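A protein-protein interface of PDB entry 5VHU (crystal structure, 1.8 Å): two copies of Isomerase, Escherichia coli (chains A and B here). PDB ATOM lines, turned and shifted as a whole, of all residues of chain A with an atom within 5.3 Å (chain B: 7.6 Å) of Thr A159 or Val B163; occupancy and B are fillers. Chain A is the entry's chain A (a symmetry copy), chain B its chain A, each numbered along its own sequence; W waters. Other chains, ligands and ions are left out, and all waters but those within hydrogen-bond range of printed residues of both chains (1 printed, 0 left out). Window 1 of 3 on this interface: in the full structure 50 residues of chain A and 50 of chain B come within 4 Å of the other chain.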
ATOM      1  N   MET A  14      25.704   5.201   9.900  1.00  0.00           N
ATOM      2  CA  MET A  14      25.475   5.912   8.625  1.00  0.00           C
ATOM      3  C   MET A  14      24.008   5.884   8.273  1.00  0.00           C
ATOM      4  O   MET A  14      23.438   6.866   7.818  1.00  0.00           O
ATOM      5  CB  MET A  14      26.272   5.305   7.475  1.00  0.00           C
ATOM      6  CG  MET A  14      27.789   5.441   7.639  1.00  0.00           C
ATOM      7  SD  MET A  14      28.674   4.903   6.157  1.00  0.00           S
ATOM      8  CE  MET A  14      28.250   6.111   4.936  1.00  0.00           C
ATOM      9  N   GLU A  17      21.897   8.343  10.219  1.00  0.00           N
ATOM     10  CA  GLU A  17      21.978   9.705   9.565  1.00  0.00           C
ATOM     11  C   GLU A  17      21.140   9.809   8.282  1.00  0.00           C
ATOM     12  O   GLU A  17      20.374  10.756   8.102  1.00  0.00           O
ATOM     13  CB  GLU A  17      23.431  10.136   9.309  1.00  0.00           C
ATOM     14  CG  GLU A  17      24.148  10.287  10.643  1.00  0.00           C
ATOM     15  CD  GLU A  17      25.375  11.180  10.567  1.00  0.00           C
ATOM     16  OE1 GLU A  17      25.587  11.883   9.549  1.00  0.00           O
ATOM     17  OE2 GLU A  17      26.118  11.180  11.548  1.00  0.00           O
ATOM     18  N   VAL A  21      17.829  12.373   7.350  1.00  0.00           N
ATOM     19  CA  VAL A  21      17.752  13.193   6.139  1.00  0.00           C
ATOM     20  C   VAL A  21      16.466  12.868   5.358  1.00  0.00           C
ATOM     21  O   VAL A  21      15.713  13.803   4.978  1.00  0.00           O
ATOM     22  CB  VAL A  21      19.011  13.085   5.261  1.00  0.00           C
ATOM     23  CG1 VAL A  21      18.856  13.922   3.992  1.00  0.00           C
ATOM     24  CG2 VAL A  21      20.255  13.604   6.025  1.00  0.00           C
ATOM     25  N   SER A 155      25.024  14.481  15.137  1.00  0.00           N
ATOM     26  CA  SER A 155      25.429  13.551  14.072  1.00  0.00           C
ATOM     27  C   SER A 155      24.251  13.600  13.085  1.00  0.00           C
ATOM     28  O   SER A 155      24.346  14.271  12.043  1.00  0.00           O
ATOM     29  CB  SER A 155      25.678  12.121  14.651  1.00  0.00           C
ATOM     30  OG  SER A 155      24.643  11.853  15.614  1.00  0.00           O
ATOM     31  N   CYS A 156      23.095  13.022  13.452  1.00  0.00           N
ATOM     32  CA  CYS A 156      21.887  13.269  12.658  1.00  0.00           C
ATOM     33  C   CYS A 156      21.574  14.773  12.533  1.00  0.00           C
ATOM     34  O   CYS A 156      21.330  15.233  11.420  1.00  0.00           O
ATOM     35  CB  CYS A 156      20.691  12.564  13.271  1.00  0.00           C
ATOM     36  SG  CYS A 156      20.914  10.778  13.286  1.00  0.00           S
ATOM     37  N   SER A 157      21.610  15.536  13.639  1.00  0.00           N
ATOM     38  CA  SER A 157      21.212  16.945  13.551  1.00  0.00           C
ATOM     39  C   SER A 157      22.178  17.793  12.690  1.00  0.00           C
ATOM     40  O   SER A 157      21.728  18.558  11.820  1.00  0.00           O
ATOM     41  CB  SER A 157      21.062  17.577  14.930  1.00  0.00           C
ATOM     42  OG  SER A 157      22.285  17.496  15.622  1.00  0.00           O
ATOM     43  N   SER A 158      23.493  17.669  12.928  1.00  0.00           N
ATOM     44  CA  SER A 158      24.454  18.449  12.118  1.00  0.00           C
ATOM     45  C   SER A 158      24.389  18.046  10.642  1.00  0.00           C
ATOM     46  O   SER A 158      24.530  18.938   9.758  1.00  0.00           O
ATOM     47  CB  SER A 158      25.891  18.326  12.724  1.00  0.00           C
ATOM     48  OG  SER A 158      26.121  16.960  13.111  1.00  0.00           O
ATOM     49  N   THR A 159      24.208  16.753  10.340  1.00  0.00           N
ATOM     50  CA  THR A 159      24.122  16.347   8.939  1.00  0.00           C
ATOM     51  C   THR A 159      22.848  16.863   8.267  1.00  0.00           C
ATOM     52  O   THR A 159      22.899  17.304   7.143  1.00  0.00           O
ATOM     53  CB  THR A 159      24.246  14.820   8.813  1.00  0.00           C
ATOM     54  OG1 THR A 159      25.586  14.484   9.200  1.00  0.00           O
ATOM     55  CG2 THR A 159      24.009  14.309   7.364  1.00  0.00           C
ATOM     56  N   VAL A 160      21.712  16.800   8.966  1.00  0.00           N
ATOM     57  CA  VAL A 160      20.492  17.277   8.379  1.00  0.00           C
ATOM     58  C   VAL A 160      20.586  18.780   8.050  1.00  0.00           C
ATOM     59  O   VAL A 160      20.119  19.225   6.991  1.00  0.00           O
ATOM     60  CB  VAL A 160      19.313  17.041   9.336  1.00  0.00           C
ATOM     61  CG1 VAL A 160      18.103  17.793   8.779  1.00  0.00           C
ATOM     62  CG2 VAL A 160      19.042  15.534   9.375  1.00  0.00           C
ATOM     63  N   VAL A 161      21.103  19.566   8.994  1.00  0.00           N
ATOM     64  CA  VAL A 161      21.270  21.027   8.757  1.00  0.00           C
ATOM     65  C   VAL A 161      22.202  21.304   7.582  1.00  0.00           C
ATOM     66  O   VAL A 161      21.950  22.228   6.772  1.00  0.00           O
ATOM     67  CB  VAL A 161      21.724  21.788  10.048  1.00  0.00           C
ATOM     68  CG1 VAL A 161      21.705  23.288   9.767  1.00  0.00           C
ATOM     69  CG2 VAL A 161      20.652  21.517  11.077  1.00  0.00           C
ATOM     70  N   LEU A 162      23.256  20.496   7.474  1.00  0.00           N
ATOM     71  CA  LEU A 162      24.170  20.672   6.339  1.00  0.00           C
ATOM     72  C   LEU A 162      23.460  20.419   4.997  1.00  0.00           C
ATOM     73  O   LEU A 162      23.629  21.182   4.043  1.00  0.00           O
ATOM     74  CB  LEU A 162      25.374  19.728   6.457  1.00  0.00           C
ATOM     75  CG  LEU A 162      26.378  19.776   5.275  1.00  0.00           C
ATOM     76  CD1 LEU A 162      26.993  21.186   5.152  1.00  0.00           C
ATOM     77  CD2 LEU A 162      27.455  18.712   5.510  1.00  0.00           C
ATOM     78  N   VAL A 163      22.698  19.351   4.940  1.00  0.00           N
ATOM     79  CA  VAL A 163      22.017  18.985   3.676  1.00  0.00           C
ATOM     80  C   VAL A 163      20.989  20.056   3.332  1.00  0.00           C
ATOM     81  O   VAL A 163      20.927  20.499   2.166  1.00  0.00           O
ATOM     82  CB  VAL A 163      21.366  17.589   3.765  1.00  0.00           C
ATOM     83  CG1 VAL A 163      20.521  17.273   2.494  1.00  0.00           C
ATOM     84  CG2 VAL A 163      22.470  16.537   3.903  1.00  0.00           C
ATOM     85  N   VAL A 164      20.215  20.479   4.327  1.00  0.00           N
ATOM     86  CA  VAL A 164      19.167  21.495   4.112  1.00  0.00           C
ATOM     87  C   VAL A 164      19.825  22.808   3.619  1.00  0.00           C
ATOM     88  O   VAL A 164      19.420  23.372   2.575  1.00  0.00           O
ATOM     89  CB  VAL A 164      18.353  21.752   5.405  1.00  0.00           C
ATOM     90  CG1 VAL A 164      17.576  23.068   5.270  1.00  0.00           C
ATOM     91  CG2 VAL A 164      17.439  20.563   5.646  1.00  0.00           C
ATOM     92  N   MET B  14      18.578  18.088  -2.141  1.00  0.00           N
ATOM     93  CA  MET B  14      18.671  17.234  -0.939  1.00  0.00           C
ATOM     94  C   MET B  14      18.732  15.781  -1.340  1.00  0.00           C
ATOM     95  O   MET B  14      19.486  14.992  -0.786  1.00  0.00           O
ATOM     96  CB  MET B  14      17.492  17.438   0.007  1.00  0.00           C
ATOM     97  CG  MET B  14      17.434  18.839   0.624  1.00  0.00           C
ATOM     98  SD  MET B  14      16.152  18.959   1.894  1.00  0.00           S
ATOM     99  CE  MET B  14      16.738  17.922   3.202  1.00  0.00           C
ATOM    100  N   GLU B  17      22.112  14.659  -2.606  1.00  0.00           N
ATOM    101  CA  GLU B  17      23.004  14.321  -1.431  1.00  0.00           C
ATOM    102  C   GLU B  17      22.660  12.972  -0.781  1.00  0.00           C
ATOM    103  O   GLU B  17      23.540  12.144  -0.540  1.00  0.00           O
ATOM    104  CB  GLU B  17      23.028  15.446  -0.384  1.00  0.00           C
ATOM    105  CG  GLU B  17      23.639  16.694  -1.006  1.00  0.00           C
ATOM    106  CD  GLU B  17      24.188  17.670   0.020  1.00  0.00           C
ATOM    107  OE1 GLU B  17      24.315  17.326   1.219  1.00  0.00           O
ATOM    108  OE2 GLU B  17      24.503  18.785  -0.395  1.00  0.00           O
ATOM    109  N   VAL B  21      25.046   9.434  -0.344  1.00  0.00           N
ATOM    110  CA  VAL B  21      25.238   8.735   0.928  1.00  0.00           C
ATOM    111  C   VAL B  21      24.816   7.260   0.795  1.00  0.00           C
ATOM    112  O   VAL B  21      25.592   6.350   1.187  1.00  0.00           O
ATOM    113  CB  VAL B  21      24.542   9.437   2.108  1.00  0.00           C
ATOM    114  CG1 VAL B  21      24.737   8.641   3.398  1.00  0.00           C
ATOM    115  CG2 VAL B  21      25.134  10.851   2.327  1.00  0.00           C
ATOM    116  N   VAL B  24      27.368   4.988  -0.837  1.00  0.00           N
ATOM    117  CA  VAL B  24      28.453   4.602   0.070  1.00  0.00           C
ATOM    118  C   VAL B  24      28.033   3.505   1.047  1.00  0.00           C
ATOM    119  O   VAL B  24      28.802   2.547   1.237  1.00  0.00           O
ATOM    120  CB  VAL B  24      29.053   5.841   0.813  1.00  0.00           C
ATOM    121  CG1 VAL B  24      30.156   5.390   1.759  1.00  0.00           C
ATOM    122  CG2 VAL B  24      29.605   6.837  -0.236  1.00  0.00           C
ATOM    123  N   ILE B  25      26.855   3.632   1.653  1.00  0.00           N
ATOM    124  CA  ILE B  25      26.306   2.606   2.579  1.00  0.00           C
ATOM    125  C   ILE B  25      26.155   1.254   1.825  1.00  0.00           C
ATOM    126  O   ILE B  25      26.334   0.210   2.414  1.00  0.00           O
ATOM    127  CB  ILE B  25      24.946   3.028   3.168  1.00  0.00           C
ATOM    128  CG1 ILE B  25      25.123   4.255   4.073  1.00  0.00           C
ATOM    129  CG2 ILE B  25      24.330   1.921   4.018  1.00  0.00           C
ATOM    130  CD1 ILE B  25      23.799   4.823   4.593  1.00  0.00           C
ATOM    131  N   ILE B  57      34.672  20.340   7.008  1.00  0.00           N
ATOM    132  CA  ILE B  57      34.229  18.970   7.473  1.00  0.00           C
ATOM    133  C   ILE B  57      35.306  18.314   8.409  1.00  0.00           C
ATOM    134  O   ILE B  57      34.958  17.727   9.444  1.00  0.00           O
ATOM    135  CB  ILE B  57      33.943  18.024   6.276  1.00  0.00           C
ATOM    136  CG1 ILE B  57      32.796  18.579   5.438  1.00  0.00           C
ATOM    137  CG2 ILE B  57      33.652  16.576   6.744  1.00  0.00           C
ATOM    138  CD1 ILE B  57      31.593  19.177   6.185  1.00  0.00           C
ATOM    139  N   LYS B  60      34.896  19.615  11.842  1.00  0.00           N
ATOM    140  CA  LYS B  60      33.744  19.007  12.511  1.00  0.00           C
ATOM    141  C   LYS B  60      34.147  17.587  12.981  1.00  0.00           C
ATOM    142  O   LYS B  60      33.883  17.211  14.161  1.00  0.00           O
ATOM    143  CB  LYS B  60      32.533  18.921  11.554  1.00  0.00           C
ATOM    144  CG  LYS B  60      31.193  18.717  12.314  1.00  0.00           C
ATOM    145  CD  LYS B  60      30.923  17.232  12.700  1.00  0.00           C
ATOM    146  CE  LYS B  60      29.472  16.991  13.160  1.00  0.00           C
ATOM    147  NZ  LYS B  60      29.298  15.560  13.679  1.00  0.00           N
ATOM    148  N   LEU B  61      34.818  16.815  12.104  1.00  0.00           N
ATOM    149  CA  LEU B  61      35.176  15.433  12.504  1.00  0.00           C
ATOM    150  C   LEU B  61      36.137  15.399  13.654  1.00  0.00           C
ATOM    151  O   LEU B  61      36.002  14.549  14.566  1.00  0.00           O
ATOM    152  CB  LEU B  61      35.760  14.668  11.290  1.00  0.00           C
ATOM    153  CG  LEU B  61      34.779  14.409  10.149  1.00  0.00           C
ATOM    154  CD1 LEU B  61      35.420  13.669   8.961  1.00  0.00           C
ATOM    155  CD2 LEU B  61      33.533  13.633  10.671  1.00  0.00           C
ATOM    156  N   SER B 157      30.012  15.484  -1.949  1.00  0.00           N
ATOM    157  CA  SER B 157      31.277  14.988  -1.397  1.00  0.00           C
ATOM    158  C   SER B 157      31.478  15.369   0.089  1.00  0.00           C
ATOM    159  O   SER B 157      31.836  14.507   0.910  1.00  0.00           O
ATOM    160  CB  SER B 157      32.474  15.459  -2.215  1.00  0.00           C
ATOM    161  OG  SER B 157      32.510  16.866  -2.233  1.00  0.00           O
ATOM    162  N   SER B 158      31.258  16.647   0.438  1.00  0.00           N
ATOM    163  CA  SER B 158      31.423  17.052   1.851  1.00  0.00           C
ATOM    164  C   SER B 158      30.420  16.331   2.754  1.00  0.00           C
ATOM    165  O   SER B 158      30.786  15.972   3.910  1.00  0.00           O
ATOM    166  CB  SER B 158      31.348  18.611   1.974  1.00  0.00           C
ATOM    167  OG  SER B 158      30.282  19.096   1.139  1.00  0.00           O
ATOM    168  N   THR B 159      29.178  16.125   2.294  1.00  0.00           N
ATOM    169  CA  THR B 159      28.209  15.419   3.131  1.00  0.00           C
ATOM    170  C   THR B 159      28.574  13.945   3.315  1.00  0.00           C
ATOM    171  O   THR B 159      28.450  13.429   4.401  1.00  0.00           O
ATOM    172  CB  THR B 159      26.789  15.582   2.563  1.00  0.00           C
ATOM    173  OG1 THR B 159      26.446  16.967   2.710  1.00  0.00           O
ATOM    174  CG2 THR B 159      25.732  14.730   3.318  1.00  0.00           C
ATOM    175  N   VAL B 160      29.018  13.280   2.246  1.00  0.00           N
ATOM    176  CA  VAL B 160      29.377  11.896   2.372  1.00  0.00           C
ATOM    177  C   VAL B 160      30.536  11.713   3.372  1.00  0.00           C
ATOM    178  O   VAL B 160      30.530  10.770   4.178  1.00  0.00           O
ATOM    179  CB  VAL B 160      29.792  11.328   1.007  1.00  0.00           C
ATOM    180  CG1 VAL B 160      30.404   9.946   1.243  1.00  0.00           C
ATOM    181  CG2 VAL B 160      28.529  11.219   0.145  1.00  0.00           C
ATOM    182  N   VAL B 161      31.563  12.553   3.255  1.00  0.00           N
ATOM    183  CA  VAL B 161      32.714  12.480   4.198  1.00  0.00           C
ATOM    184  C   VAL B 161      32.278  12.726   5.638  1.00  0.00           C
ATOM    185  O   VAL B 161      32.770  12.055   6.576  1.00  0.00           O
ATOM    186  CB  VAL B 161      33.884  13.430   3.777  1.00  0.00           C
ATOM    187  CG1 VAL B 161      35.081  13.171   4.688  1.00  0.00           C
ATOM    188  CG2 VAL B 161      34.284  12.993   2.387  1.00  0.00           C
ATOM    189  N   LEU B 162      31.345  13.662   5.811  1.00  0.00           N
ATOM    190  CA  LEU B 162      30.841  13.918   7.166  1.00  0.00           C
ATOM    191  C   LEU B 162      30.136  12.680   7.750  1.00  0.00           C
ATOM    192  O   LEU B 162      30.352  12.323   8.911  1.00  0.00           O
ATOM    193  CB  LEU B 162      29.865  15.102   7.170  1.00  0.00           C
ATOM    194  CG  LEU B 162      29.213  15.425   8.540  1.00  0.00           C
ATOM    195  CD1 LEU B 162      30.296  15.803   9.572  1.00  0.00           C
ATOM    196  CD2 LEU B 162      28.205  16.560   8.342  1.00  0.00           C
ATOM    197  N   VAL B 163      29.298  12.062   6.950  1.00  0.00           N
ATOM    198  CA  VAL B 163      28.524  10.896   7.434  1.00  0.00           C
ATOM    199  C   VAL B 163      29.482   9.751   7.742  1.00  0.00           C
ATOM    200  O   VAL B 163      29.360   9.115   8.809  1.00  0.00           O
ATOM    201  CB  VAL B 163      27.444  10.469   6.420  1.00  0.00           C
ATOM    202  CG1 VAL B 163      26.738   9.151   6.860  1.00  0.00           C
ATOM    203  CG2 VAL B 163      26.399  11.582   6.312  1.00  0.00           C
ATOM    204  N   VAL B 164      30.426   9.508   6.837  1.00  0.00           N
ATOM    205  CA  VAL B 164      31.397   8.410   7.011  1.00  0.00           C
ATOM    206  C   VAL B 164      32.222   8.659   8.299  1.00  0.00           C
ATOM    207  O   VAL B 164      32.318   7.770   9.177  1.00  0.00           O
ATOM    208  CB  VAL B 164      32.335   8.284   5.784  1.00  0.00           C
ATOM    209  CG1 VAL B 164      33.560   7.440   6.159  1.00  0.00           C
ATOM    210  CG2 VAL B 164      31.549   7.682   4.633  1.00  0.00           C
ATOM    211  N   GLY B 165      32.785   9.863   8.423  1.00  0.00           N
ATOM    212  CA  GLY B 165      33.577  10.224   9.604  1.00  0.00           C
ATOM    213  C   GLY B 165      32.815  10.164  10.920  1.00  0.00           C
ATOM    214  O   GLY B 165      33.374   9.690  11.934  1.00  0.00           O
ATOM    215  N   ASP B 166      31.562  10.657  10.935  1.00  0.00           N
ATOM    216  CA  ASP B 166      30.727  10.571  12.150  1.00  0.00           C
ATOM    217  C   ASP B 166      30.587   9.074  12.572  1.00  0.00           C
ATOM    218  O   ASP B 166      30.702   8.722  13.757  1.00  0.00           O
ATOM    219  CB  ASP B 166      29.331  11.079  11.921  1.00  0.00           C
ATOM    220  CG  ASP B 166      29.186  12.552  12.047  1.00  0.00           C
ATOM    221  OD1 ASP B 166      30.177  13.292  12.422  1.00  0.00           O
ATOM    222  OD2 ASP B 166      27.998  13.014  11.787  1.00  0.00           O
ATOM    223  N   ALA B 167      30.328   8.216  11.573  1.00  0.00           N
ATOM    224  CA  ALA B 167      30.110   6.785  11.895  1.00  0.00           C
ATOM    225  C   ALA B 167      31.365   6.146  12.434  1.00  0.00           C
ATOM    226  O   ALA B 167      31.288   5.315  13.349  1.00  0.00           O
ATOM    227  CB  ALA B 167      29.613   6.083  10.653  1.00  0.00           C
ATOM    228  N   VAL B 168      32.527   6.499  11.861  1.00  0.00           N
ATOM    229  CA  VAL B 168      33.821   5.995  12.359  1.00  0.00           C
ATOM    230  C   VAL B 168      33.999   6.460  13.817  1.00  0.00           C
ATOM    231  O   VAL B 168      34.336   5.646  14.688  1.00  0.00           O
ATOM    232  CB  VAL B 168      34.992   6.454  11.470  1.00  0.00           C
ATOM    233  CG1 VAL B 168      36.317   6.140  12.164  1.00  0.00           C
ATOM    234  CG2 VAL B 168      34.894   5.688  10.158  1.00  0.00           C
ATOM    235  N   ALA B 169      33.743   7.750  14.100  1.00  0.00           N
ATOM    236  CA  ALA B 169      33.829   8.273  15.468  1.00  0.00           C
ATOM    237  C   ALA B 169      32.921   7.490  16.425  1.00  0.00           C
ATOM    238  O   ALA B 169      33.358   7.088  17.518  1.00  0.00           O
ATOM    239  CB  ALA B 169      33.453   9.783  15.474  1.00  0.00           C
ATOM    240  N   LEU B 170      31.662   7.289  16.026  1.00  0.00           N
ATOM    241  CA  LEU B 170      30.692   6.644  16.929  1.00  0.00           C
ATOM    242  C   LEU B 170      31.027   5.167  17.129  1.00  0.00           C
ATOM    243  O   LEU B 170      30.830   4.618  18.231  1.00  0.00           O
ATOM    244  CB  LEU B 170      29.247   6.825  16.441  1.00  0.00           C
ATOM    245  CG  LEU B 170      28.728   8.292  16.477  1.00  0.00           C
ATOM    246  CD1 LEU B 170      27.288   8.412  15.934  1.00  0.00           C
ATOM    247  CD2 LEU B 170      28.893   9.009  17.833  1.00  0.00           C
HETATM  248  O   HOH W   1      27.183  15.456  11.367  1.00  0.00           O
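Of the printed residues of chain B, Met A14 touches Val B24, Ile B25, Val B163, Val B164 and Ala B167. Of chain B, only Lys B60 (3.4 Å) comes within 4 Å of Ser A158. Ile B57 touches none of the printed residues of chain A. Printed residues of chain A within 4 Å of Val B163: Met A14 (3.9 Å), Glu A17 (3.4 Å) and Thr A159 (3.8 Å). Of the printed residues of chain A, Asp B166 touches Glu A17, Ser A155 and Thr A159. Of the printed residues of chain A, Ala B167 touches Met A14 (3.6 Å).
Met A14 touches Val B164, and with the chains exchanged Val A164 touches Met B14. Glu A17 touches Val B163, and with the chains exchanged Val A163 touches Glu B17. Thr A159 touches Leu B162, and with the chains exchanged Leu A162 touches Thr B159. Thr A159 touches Val B163, and with the chains exchanged Val A163 touches Thr B159. Positions printed for both chains: 14, 17, 21, 157, 158, 159, 160, 161, 162, 163 and 164. Of the 18 pairs that touch across the chains among the printed residues, 11 have their exchanged pair printed and touching as well.
The side-chain carboxylate (OD2) of Asp B166 sits close to the side-chain carboxylate (OE2) of Glu A17.
OG1 of Thr B159 sits at hydrogen-bond distance from OE1 of Glu B17, at 2.6 Å. The side-chain amino group (NZ) of Lys B60 is in salt-bridge range of the side-chain carboxylate (OD1) of Asp B166, at 2.7 Å. OG1 of Thr A159 sits at hydrogen-bond distance from OE1 of Glu A17 (2.6 Å). OG of Ser A158 is in hydrogen-bond range of N of Ser A155, at 3.4 Å. OG1 of Thr A159 is in hydrogen-bond range of O of Ser A155 (3.1 Å).
Among the printed residues, no Asp or Glu carboxylate lies within 4 Å of a Lys or Arg side-chain nitrogen of the other chain.
Among the printed residues, merely in contact across the chains: Glu A17 with Val B163, Val A163 with Glu B17, Ser A158 with Lys B60, Leu A162 with Thr B159, Thr A159 with Leu B162, Ser A155 with Asp B166, Met A14 with Ala B167, Leu A162 with Leu B162, Val A164 with Met B14, Met A14 with Val B164, Met A14 with Ile B25, Met A14 with Val B24, Val A163 with Thr B159, Thr A159 with Val B163, Thr A159 with Asp B166, Met A14 with Val B163 and Val A163 with Met B14.
Water W1 lies within hydrogen-bond range of the side-chain hydroxyl of Ser A158, the side-chain carboxylate of Asp B166, the side-chain hydroxyl of Thr A159, the side-chain amino group of Lys B60 and the backbone carbonyl oxygen of Ser A155.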
